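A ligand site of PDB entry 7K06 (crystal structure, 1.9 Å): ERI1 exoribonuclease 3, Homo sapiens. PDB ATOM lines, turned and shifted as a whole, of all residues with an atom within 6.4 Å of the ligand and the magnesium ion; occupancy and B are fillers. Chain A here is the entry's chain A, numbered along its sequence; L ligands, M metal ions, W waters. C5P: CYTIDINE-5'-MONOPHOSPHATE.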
ATOM      1  N   ASP A  29      -3.834 -10.706  -0.765  1.00  0.00           N
ATOM      2  CA  ASP A  29      -4.414 -11.702   0.135  1.00  0.00           C
ATOM      3  C   ASP A  29      -5.930 -11.690  -0.065  1.00  0.00           C
ATOM      4  O   ASP A  29      -6.614 -10.823   0.480  1.00  0.00           O
ATOM      5  CB  ASP A  29      -4.051 -11.408   1.581  1.00  0.00           C
ATOM      6  CG  ASP A  29      -4.249 -12.613   2.488  1.00  0.00           C
ATOM      7  OD1 ASP A  29      -3.244 -13.269   2.847  1.00  0.00           O
ATOM      8  OD2 ASP A  29      -5.407 -12.910   2.839  1.00  0.00           O
ATOM      9  N   PHE A  30      -6.438 -12.643  -0.836  1.00  0.00           N
ATOM     10  CA  PHE A  30      -7.869 -12.714  -1.100  1.00  0.00           C
ATOM     11  C   PHE A  30      -8.644 -13.086   0.151  1.00  0.00           C
ATOM     12  O   PHE A  30      -8.125 -13.759   1.054  1.00  0.00           O
ATOM     13  CB  PHE A  30      -8.168 -13.756  -2.178  1.00  0.00           C
ATOM     14  CG  PHE A  30      -7.653 -13.410  -3.541  1.00  0.00           C
ATOM     15  CD1 PHE A  30      -7.842 -12.152  -4.085  1.00  0.00           C
ATOM     16  CD2 PHE A  30      -6.975 -14.369  -4.283  1.00  0.00           C
ATOM     17  CE1 PHE A  30      -7.364 -11.854  -5.350  1.00  0.00           C
ATOM     18  CE2 PHE A  30      -6.497 -14.071  -5.549  1.00  0.00           C
ATOM     19  CZ  PHE A  30      -6.689 -12.813  -6.078  1.00  0.00           C
ATOM     20  N   GLU A  31      -9.902 -12.666   0.202  1.00  0.00           N
ATOM     21  CA  GLU A  31     -10.923 -13.344   0.974  1.00  0.00           C
ATOM     22  C   GLU A  31     -11.971 -13.851   0.005  1.00  0.00           C
ATOM     23  O   GLU A  31     -12.214 -13.236  -1.036  1.00  0.00           O
ATOM     24  CB  GLU A  31     -11.558 -12.437   2.031  1.00  0.00           C
ATOM     25  CG  GLU A  31     -10.561 -11.825   3.011  1.00  0.00           C
ATOM     26  CD  GLU A  31      -9.758 -12.862   3.777  1.00  0.00           C
ATOM     27  OE1 GLU A  31     -10.256 -13.985   4.009  1.00  0.00           O
ATOM     28  OE2 GLU A  31      -8.616 -12.533   4.156  1.00  0.00           O
ATOM     29  N   ALA A  32     -12.584 -14.994   0.332  1.00  0.00           N
ATOM     30  CA  ALA A  32     -13.513 -15.647  -0.576  1.00  0.00           C
ATOM     31  C   ALA A  32     -14.735 -16.115   0.201  1.00  0.00           C
ATOM     32  O   ALA A  32     -14.684 -16.306   1.415  1.00  0.00           O
ATOM     33  CB  ALA A  32     -12.860 -16.852  -1.283  1.00  0.00           C
ATOM     34  N   THR A  33     -15.845 -16.291  -0.529  1.00  0.00           N
ATOM     35  CA  THR A  33     -17.013 -16.942   0.055  1.00  0.00           C
ATOM     36  C   THR A  33     -16.614 -18.280   0.658  1.00  0.00           C
ATOM     37  O   THR A  33     -15.716 -18.972   0.163  1.00  0.00           O
ATOM     38  CB  THR A  33     -18.099 -17.179  -0.998  1.00  0.00           C
ATOM     39  OG1 THR A  33     -17.575 -17.994  -2.060  1.00  0.00           O
ATOM     40  CG2 THR A  33     -18.611 -15.847  -1.571  1.00  0.00           C
ATOM     41  N   CYS A  34     -17.277 -18.660   1.736  1.00  0.00           N
ATOM     42  CA  CYS A  34     -16.928 -19.873   2.444  1.00  0.00           C
ATOM     43  C   CYS A  34     -18.127 -20.321   3.274  1.00  0.00           C
ATOM     44  O   CYS A  34     -19.148 -19.633   3.351  1.00  0.00           O
ATOM     45  CB  CYS A  34     -15.688 -19.660   3.311  1.00  0.00           C
ATOM     46  SG  CYS A  34     -15.790 -18.203   4.349  1.00  0.00           S
ATOM     47  N   ASP A  35     -17.975 -21.495   3.899  1.00  0.00           N
ATOM     48  CA  ASP A  35     -18.980 -22.078   4.775  1.00  0.00           C
ATOM     49  C   ASP A  35     -18.330 -23.259   5.479  1.00  0.00           C
ATOM     50  O   ASP A  35     -17.162 -23.593   5.225  1.00  0.00           O
ATOM     51  CB  ASP A  35     -20.230 -22.498   3.986  1.00  0.00           C
ATOM     52  CG  ASP A  35     -21.484 -22.534   4.849  1.00  0.00           C
ATOM     53  OD1 ASP A  35     -21.386 -22.289   6.068  1.00  0.00           O
ATOM     54  OD2 ASP A  35     -22.573 -22.790   4.294  1.00  0.00           O
ATOM     55  N   LYS A  36     -19.091 -23.901   6.363  1.00  0.00           N
ATOM     56  CA  LYS A  36     -18.678 -25.151   6.998  1.00  0.00           C
ATOM     57  C   LYS A  36     -19.845 -26.117   6.912  1.00  0.00           C
ATOM     58  O   LYS A  36     -20.892 -25.866   7.534  1.00  0.00           O
ATOM     59  CB  LYS A  36     -18.236 -24.925   8.443  1.00  0.00           C
ATOM     60  CG  LYS A  36     -16.923 -24.153   8.570  1.00  0.00           C
ATOM     61  CD  LYS A  36     -15.740 -24.981   8.058  1.00  0.00           C
ATOM     62  CE  LYS A  36     -14.467 -24.152   7.929  1.00  0.00           C
ATOM     63  NZ  LYS A  36     -14.384 -23.405   6.636  1.00  0.00           N
ATOM     64  N   GLN A  38     -17.231 -26.652   3.490  1.00  0.00           N
ATOM     65  CA  GLN A  38     -16.813 -25.581   2.598  1.00  0.00           C
ATOM     66  C   GLN A  38     -17.782 -25.410   1.437  1.00  0.00           C
ATOM     67  O   GLN A  38     -18.285 -26.383   0.863  1.00  0.00           O
ATOM     68  CB  GLN A  38     -15.397 -25.859   2.076  1.00  0.00           C
ATOM     69  CG  GLN A  38     -14.763 -24.692   1.348  1.00  0.00           C
ATOM     70  CD  GLN A  38     -14.828 -23.406   2.153  1.00  0.00           C
ATOM     71  OE1 GLN A  38     -15.850 -22.726   2.157  1.00  0.00           O
ATOM     72  NE2 GLN A  38     -13.740 -23.075   2.839  1.00  0.00           N
ATOM     73  N   GLN A  42     -15.946 -21.645  -4.379  1.00  0.00           N
ATOM     74  CA  GLN A  42     -15.613 -20.415  -3.697  1.00  0.00           C
ATOM     75  C   GLN A  42     -15.455 -19.289  -4.706  1.00  0.00           C
ATOM     76  O   GLN A  42     -15.126 -19.527  -5.875  1.00  0.00           O
ATOM     77  CB  GLN A  42     -14.322 -20.568  -2.895  1.00  0.00           C
ATOM     78  CG  GLN A  42     -14.446 -21.483  -1.684  1.00  0.00           C
ATOM     79  CD  GLN A  42     -13.186 -21.473  -0.835  1.00  0.00           C
ATOM     80  OE1 GLN A  42     -12.294 -22.297  -1.027  1.00  0.00           O
ATOM     81  NE2 GLN A  42     -13.098 -20.525   0.088  1.00  0.00           N
ATOM     82  N   ILE A  45     -14.223 -12.380  -2.810  1.00  0.00           N
ATOM     83  CA  ILE A  45     -15.056 -11.263  -2.354  1.00  0.00           C
ATOM     84  C   ILE A  45     -14.261 -10.055  -1.872  1.00  0.00           C
ATOM     85  O   ILE A  45     -14.857  -9.004  -1.662  1.00  0.00           O
ATOM     86  CB  ILE A  45     -16.050 -11.698  -1.248  1.00  0.00           C
ATOM     87  CG1 ILE A  45     -15.321 -12.231  -0.027  1.00  0.00           C
ATOM     88  CG2 ILE A  45     -17.048 -12.703  -1.797  1.00  0.00           C
ATOM     89  CD1 ILE A  45     -16.245 -12.577   1.123  1.00  0.00           C
ATOM     90  N   PHE A  78     -21.106 -17.998   8.506  1.00  0.00           N
ATOM     91  CA  PHE A  78     -19.702 -18.324   8.729  1.00  0.00           C
ATOM     92  C   PHE A  78     -18.791 -17.344   8.001  1.00  0.00           C
ATOM     93  O   PHE A  78     -17.811 -16.839   8.575  1.00  0.00           O
ATOM     94  CB  PHE A  78     -19.402 -19.756   8.288  1.00  0.00           C
ATOM     95  CG  PHE A  78     -17.950 -20.107   8.385  1.00  0.00           C
ATOM     96  CD1 PHE A  78     -17.405 -20.499   9.590  1.00  0.00           C
ATOM     97  CD2 PHE A  78     -17.128 -19.997   7.284  1.00  0.00           C
ATOM     98  CE1 PHE A  78     -16.066 -20.798   9.690  1.00  0.00           C
ATOM     99  CE2 PHE A  78     -15.782 -20.285   7.377  1.00  0.00           C
ATOM    100  CZ  PHE A  78     -15.250 -20.690   8.581  1.00  0.00           C
ATOM    101  N   CYS A  79     -19.093 -17.058   6.741  1.00  0.00           N
ATOM    102  CA  CYS A  79     -18.240 -16.176   5.951  1.00  0.00           C
ATOM    103  C   CYS A  79     -18.153 -14.791   6.569  1.00  0.00           C
ATOM    104  O   CYS A  79     -17.064 -14.222   6.697  1.00  0.00           O
ATOM    105  CB  CYS A  79     -18.766 -16.089   4.519  1.00  0.00           C
ATOM    106  SG  CYS A  79     -17.904 -14.883   3.492  1.00  0.00           S
ATOM    107  N   LEU A  82     -16.151 -15.058   9.792  1.00  0.00           N
ATOM    108  CA  LEU A  82     -14.728 -15.282   9.585  1.00  0.00           C
ATOM    109  C   LEU A  82     -14.028 -14.016   9.122  1.00  0.00           C
ATOM    110  O   LEU A  82     -13.007 -13.607   9.689  1.00  0.00           O
ATOM    111  CB  LEU A  82     -14.512 -16.401   8.566  1.00  0.00           C
ATOM    112  CG  LEU A  82     -13.044 -16.717   8.288  1.00  0.00           C
ATOM    113  CD1 LEU A  82     -12.419 -17.422   9.494  1.00  0.00           C
ATOM    114  CD2 LEU A  82     -12.910 -17.560   7.017  1.00  0.00           C
ATOM    115  N   THR A  83     -14.564 -13.381   8.067  1.00  0.00           N
ATOM    116  CA  THR A  83     -13.893 -12.273   7.400  1.00  0.00           C
ATOM    117  C   THR A  83     -14.323 -10.908   7.907  1.00  0.00           C
ATOM    118  O   THR A  83     -13.619  -9.925   7.652  1.00  0.00           O
ATOM    119  CB  THR A  83     -14.175 -12.325   5.894  1.00  0.00           C
ATOM    120  OG1 THR A  83     -15.563 -12.079   5.666  1.00  0.00           O
ATOM    121  CG2 THR A  83     -13.801 -13.687   5.326  1.00  0.00           C
ATOM    122  N   TRP A 127      -2.062 -20.496  -2.114  1.00  0.00           N
ATOM    123  CA  TRP A 127      -3.463 -20.732  -2.448  1.00  0.00           C
ATOM    124  C   TRP A 127      -4.026 -19.638  -3.353  1.00  0.00           C
ATOM    125  O   TRP A 127      -4.750 -19.935  -4.319  1.00  0.00           O
ATOM    126  CB  TRP A 127      -4.281 -20.833  -1.166  1.00  0.00           C
ATOM    127  CG  TRP A 127      -5.756 -21.001  -1.403  1.00  0.00           C
ATOM    128  CD1 TRP A 127      -6.395 -22.148  -1.759  1.00  0.00           C
ATOM    129  CD2 TRP A 127      -6.773 -20.000  -1.276  1.00  0.00           C
ATOM    130  NE1 TRP A 127      -7.747 -21.916  -1.886  1.00  0.00           N
ATOM    131  CE2 TRP A 127      -7.999 -20.602  -1.587  1.00  0.00           C
ATOM    132  CE3 TRP A 127      -6.752 -18.635  -0.930  1.00  0.00           C
ATOM    133  CZ2 TRP A 127      -9.203 -19.910  -1.560  1.00  0.00           C
ATOM    134  CZ3 TRP A 127      -7.951 -17.953  -0.915  1.00  0.00           C
ATOM    135  CH2 TRP A 127      -9.158 -18.581  -1.220  1.00  0.00           C
ATOM    136  N   ASP A 128      -3.695 -18.379  -3.070  1.00  0.00           N
ATOM    137  CA  ASP A 128      -4.361 -17.267  -3.736  1.00  0.00           C
ATOM    138  C   ASP A 128      -4.169 -17.309  -5.248  1.00  0.00           C
ATOM    139  O   ASP A 128      -5.124 -17.197  -6.013  1.00  0.00           O
ATOM    140  CB  ASP A 128      -3.850 -15.947  -3.172  1.00  0.00           C
ATOM    141  CG  ASP A 128      -4.061 -15.860  -1.681  1.00  0.00           C
ATOM    142  OD1 ASP A 128      -4.965 -15.115  -1.255  1.00  0.00           O
ATOM    143  OD2 ASP A 128      -3.341 -16.565  -0.933  1.00  0.00           O
ATOM    144  N   LEU A 170       0.553 -16.248   9.089  1.00  0.00           N
ATOM    145  CA  LEU A 170       0.969 -14.918   9.520  1.00  0.00           C
ATOM    146  C   LEU A 170       1.106 -14.839  11.033  1.00  0.00           C
ATOM    147  O   LEU A 170       1.994 -14.143  11.540  1.00  0.00           O
ATOM    148  CB  LEU A 170      -0.023 -13.865   9.027  1.00  0.00           C
ATOM    149  CG  LEU A 170      -0.177 -13.711   7.523  1.00  0.00           C
ATOM    150  CD1 LEU A 170      -1.246 -12.676   7.198  1.00  0.00           C
ATOM    151  CD2 LEU A 170       1.155 -13.351   6.904  1.00  0.00           C
ATOM    152  N   PRO A 185      -7.400 -10.519  11.801  1.00  0.00           N
ATOM    153  CA  PRO A 185      -7.133 -11.692  10.968  1.00  0.00           C
ATOM    154  C   PRO A 185      -8.298 -12.000  10.035  1.00  0.00           C
ATOM    155  O   PRO A 185      -9.459 -11.788  10.386  1.00  0.00           O
ATOM    156  CB  PRO A 185      -6.918 -12.824  11.983  1.00  0.00           C
ATOM    157  CG  PRO A 185      -6.485 -12.109  13.240  1.00  0.00           C
ATOM    158  CD  PRO A 185      -7.264 -10.826  13.240  1.00  0.00           C
ATOM    159  N   HIS A 186      -7.975 -12.487   8.839  1.00  0.00           N
ATOM    160  CA  HIS A 186      -8.919 -12.842   7.778  1.00  0.00           C
ATOM    161  C   HIS A 186      -9.612 -11.616   7.178  1.00  0.00           C
ATOM    162  O   HIS A 186     -10.601 -11.772   6.448  1.00  0.00           O
ATOM    163  CB  HIS A 186      -9.955 -13.859   8.254  1.00  0.00           C
ATOM    164  CG  HIS A 186      -9.366 -15.043   8.940  1.00  0.00           C
ATOM    165  ND1 HIS A 186      -8.717 -16.053   8.254  1.00  0.00           N
ATOM    166  CD2 HIS A 186      -9.297 -15.375  10.246  1.00  0.00           C
ATOM    167  CE1 HIS A 186      -8.278 -16.959   9.115  1.00  0.00           C
ATOM    168  NE2 HIS A 186      -8.628 -16.577  10.328  1.00  0.00           N
ATOM    169  N   SER A 187      -9.144 -10.411   7.491  1.00  0.00           N
ATOM    170  CA  SER A 187      -9.439  -9.241   6.681  1.00  0.00           C
ATOM    171  C   SER A 187      -8.355  -9.163   5.617  1.00  0.00           C
ATOM    172  O   SER A 187      -7.166  -9.148   5.948  1.00  0.00           O
ATOM    173  CB  SER A 187      -9.464  -7.964   7.523  1.00  0.00           C
ATOM    174  OG  SER A 187      -9.358  -6.817   6.704  1.00  0.00           O
ATOM    175  N   GLY A 188      -8.759  -9.140   4.350  1.00  0.00           N
ATOM    176  CA  GLY A 188      -7.771  -9.162   3.275  1.00  0.00           C
ATOM    177  C   GLY A 188      -6.763  -8.038   3.384  1.00  0.00           C
ATOM    178  O   GLY A 188      -5.555  -8.260   3.361  1.00  0.00           O
ATOM    179  N   ASP A 191      -4.550  -8.523   6.425  1.00  0.00           N
ATOM    180  CA  ASP A 191      -3.567  -9.572   6.172  1.00  0.00           C
ATOM    181  C   ASP A 191      -2.425  -9.026   5.310  1.00  0.00           C
ATOM    182  O   ASP A 191      -1.252  -9.348   5.553  1.00  0.00           O
ATOM    183  CB  ASP A 191      -4.234 -10.769   5.490  1.00  0.00           C
ATOM    184  CG  ASP A 191      -5.062 -11.607   6.461  1.00  0.00           C
ATOM    185  OD1 ASP A 191      -4.928 -11.405   7.691  1.00  0.00           O
ATOM    186  OD2 ASP A 191      -5.832 -12.462   5.995  1.00  0.00           O
HETATM  187  O3P C5P L   1      -6.756 -17.051   5.982  1.00  0.00           O
HETATM  188  P   C5P L   1      -7.530 -16.325   4.934  1.00  0.00           P
HETATM  189  O1P C5P L   1      -6.683 -15.585   3.958  1.00  0.00           O
HETATM  190  O2P C5P L   1      -8.605 -15.435   5.469  1.00  0.00           O
HETATM  191  O5' C5P L   1      -8.199 -17.536   4.108  1.00  0.00           O
HETATM  192  C5' C5P L   1      -8.663 -17.389   2.755  1.00  0.00           C
HETATM  193  C4' C5P L   1     -10.084 -17.898   2.582  1.00  0.00           C
HETATM  194  O4' C5P L   1     -10.159 -19.304   2.920  1.00  0.00           O
HETATM  195  C3' C5P L   1     -11.176 -17.235   3.425  1.00  0.00           C
HETATM  196  O3' C5P L   1     -11.664 -16.032   2.851  1.00  0.00           O
HETATM  197  C2' C5P L   1     -12.240 -18.331   3.483  1.00  0.00           C
HETATM  198  O2' C5P L   1     -12.977 -18.330   2.263  1.00  0.00           O
HETATM  199  C1' C5P L   1     -11.401 -19.598   3.537  1.00  0.00           C
HETATM  200  N1  C5P L   1     -11.245 -20.057   4.947  1.00  0.00           N
HETATM  201  C2  C5P L   1     -12.264 -20.854   5.462  1.00  0.00           C
HETATM  202  N3  C5P L   1     -12.141 -21.273   6.726  1.00  0.00           N
HETATM  203  C4  C5P L   1     -11.112 -20.984   7.498  1.00  0.00           C
HETATM  204  C5  C5P L   1     -10.037 -20.168   6.979  1.00  0.00           C
HETATM  205  C6  C5P L   1     -10.142 -19.735   5.723  1.00  0.00           C
HETATM  206  O2  C5P L   1     -13.205 -21.113   4.733  1.00  0.00           O
HETATM  207  N4  C5P L   1     -11.072 -21.449   8.743  1.00  0.00           N
HETATM  208 MG    MG M   1      -6.738 -13.399   4.175  1.00  0.00          MG
HETATM  209  O   HOH W   1      -5.502 -14.816   7.141  1.00  0.00           O
HETATM  210  O   HOH W   2      -6.764 -19.559   4.046  1.00  0.00           O
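NE2 of Gln 38 is in hydrogen-bond range of O2 of the ligand (2.8 Å). O3' of the ligand lies within hydrogen-bond range of N of Ala 32, at 2.9 Å. The backbone carbonyl oxygen (O) of Ala 32 is in hydrogen-bond range of an oxygen (O2') of the ligand (2.8 Å). An oxygen (O2P) of the ligand lies within hydrogen-bond range of a ring nitrogen (ND1) of His 186, at 2.9 Å. An oxygen (O2') of the ligand sits at hydrogen-bond distance from the side-chain amide nitrogen (NE2) of Gln 42 (3.1 Å). The side-chain amino group (NZ) of Lys 36 lies within hydrogen-bond range of a nitrogen (N3) of the ligand (3.1 Å). O2' of the ligand sits close to SG of Cys 34.
Merely in contact with the ligand: Phe 30, Thr 33, Phe 78, Leu 82 and Trp 127. Hydrophobic or aromatic side chains that line the ligand: Ala 32, Phe 78, Leu 82, Trp 127 and His 186. Of the 23 residues printed, 14 come within 4 Å of the ligand. The nearest printed residue that does not touch the ligand is Thr 83 (4.02 Å).
Phe 30 touches the magnesium ion (O to MG, 3.4 Å). Of the 23 residues printed, 4 come within 4 Å of the magnesium ion. The nearest printed residue that does not touch the magnesium ion is His 186 (4.2 Å).
The magnesium ion is bound by OD2 of Asp 29, OE2 of Glu 31, O1P of the ligand and OD2 of Asp 191. The magnesium ion has four donor atoms within binding distance.
The side-chain carboxylate (OE2) of Glu 31 lies close to the backbone NH (N) of Gly 188, 3.4 Å away. O of Glu 31 sits at hydrogen-bond distance from N of Ile 45 (2.8 Å). The side-chain carboxylate (OD1) of Asp 191 sits at hydrogen-bond distance from the backbone NH (N) of His 186 (3.4 Å). The side-chain amide oxygen (OE1) of Gln 38 sits at hydrogen-bond distance from the backbone NH (N) of Asp 35, 3.0 Å away. The backbone carbonyl oxygen of Ala 32 lies within hydrogen-bond range of the side-chain sulfur of Cys 34, 3.7 Å away. NE2 of Gln 42 is in hydrogen-bond range of O of Thr 33, at 3.0 Å. The backbone NH of Phe 30 lies within hydrogen-bond range of the side-chain carboxylate of Asp 128 (2.9 Å).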
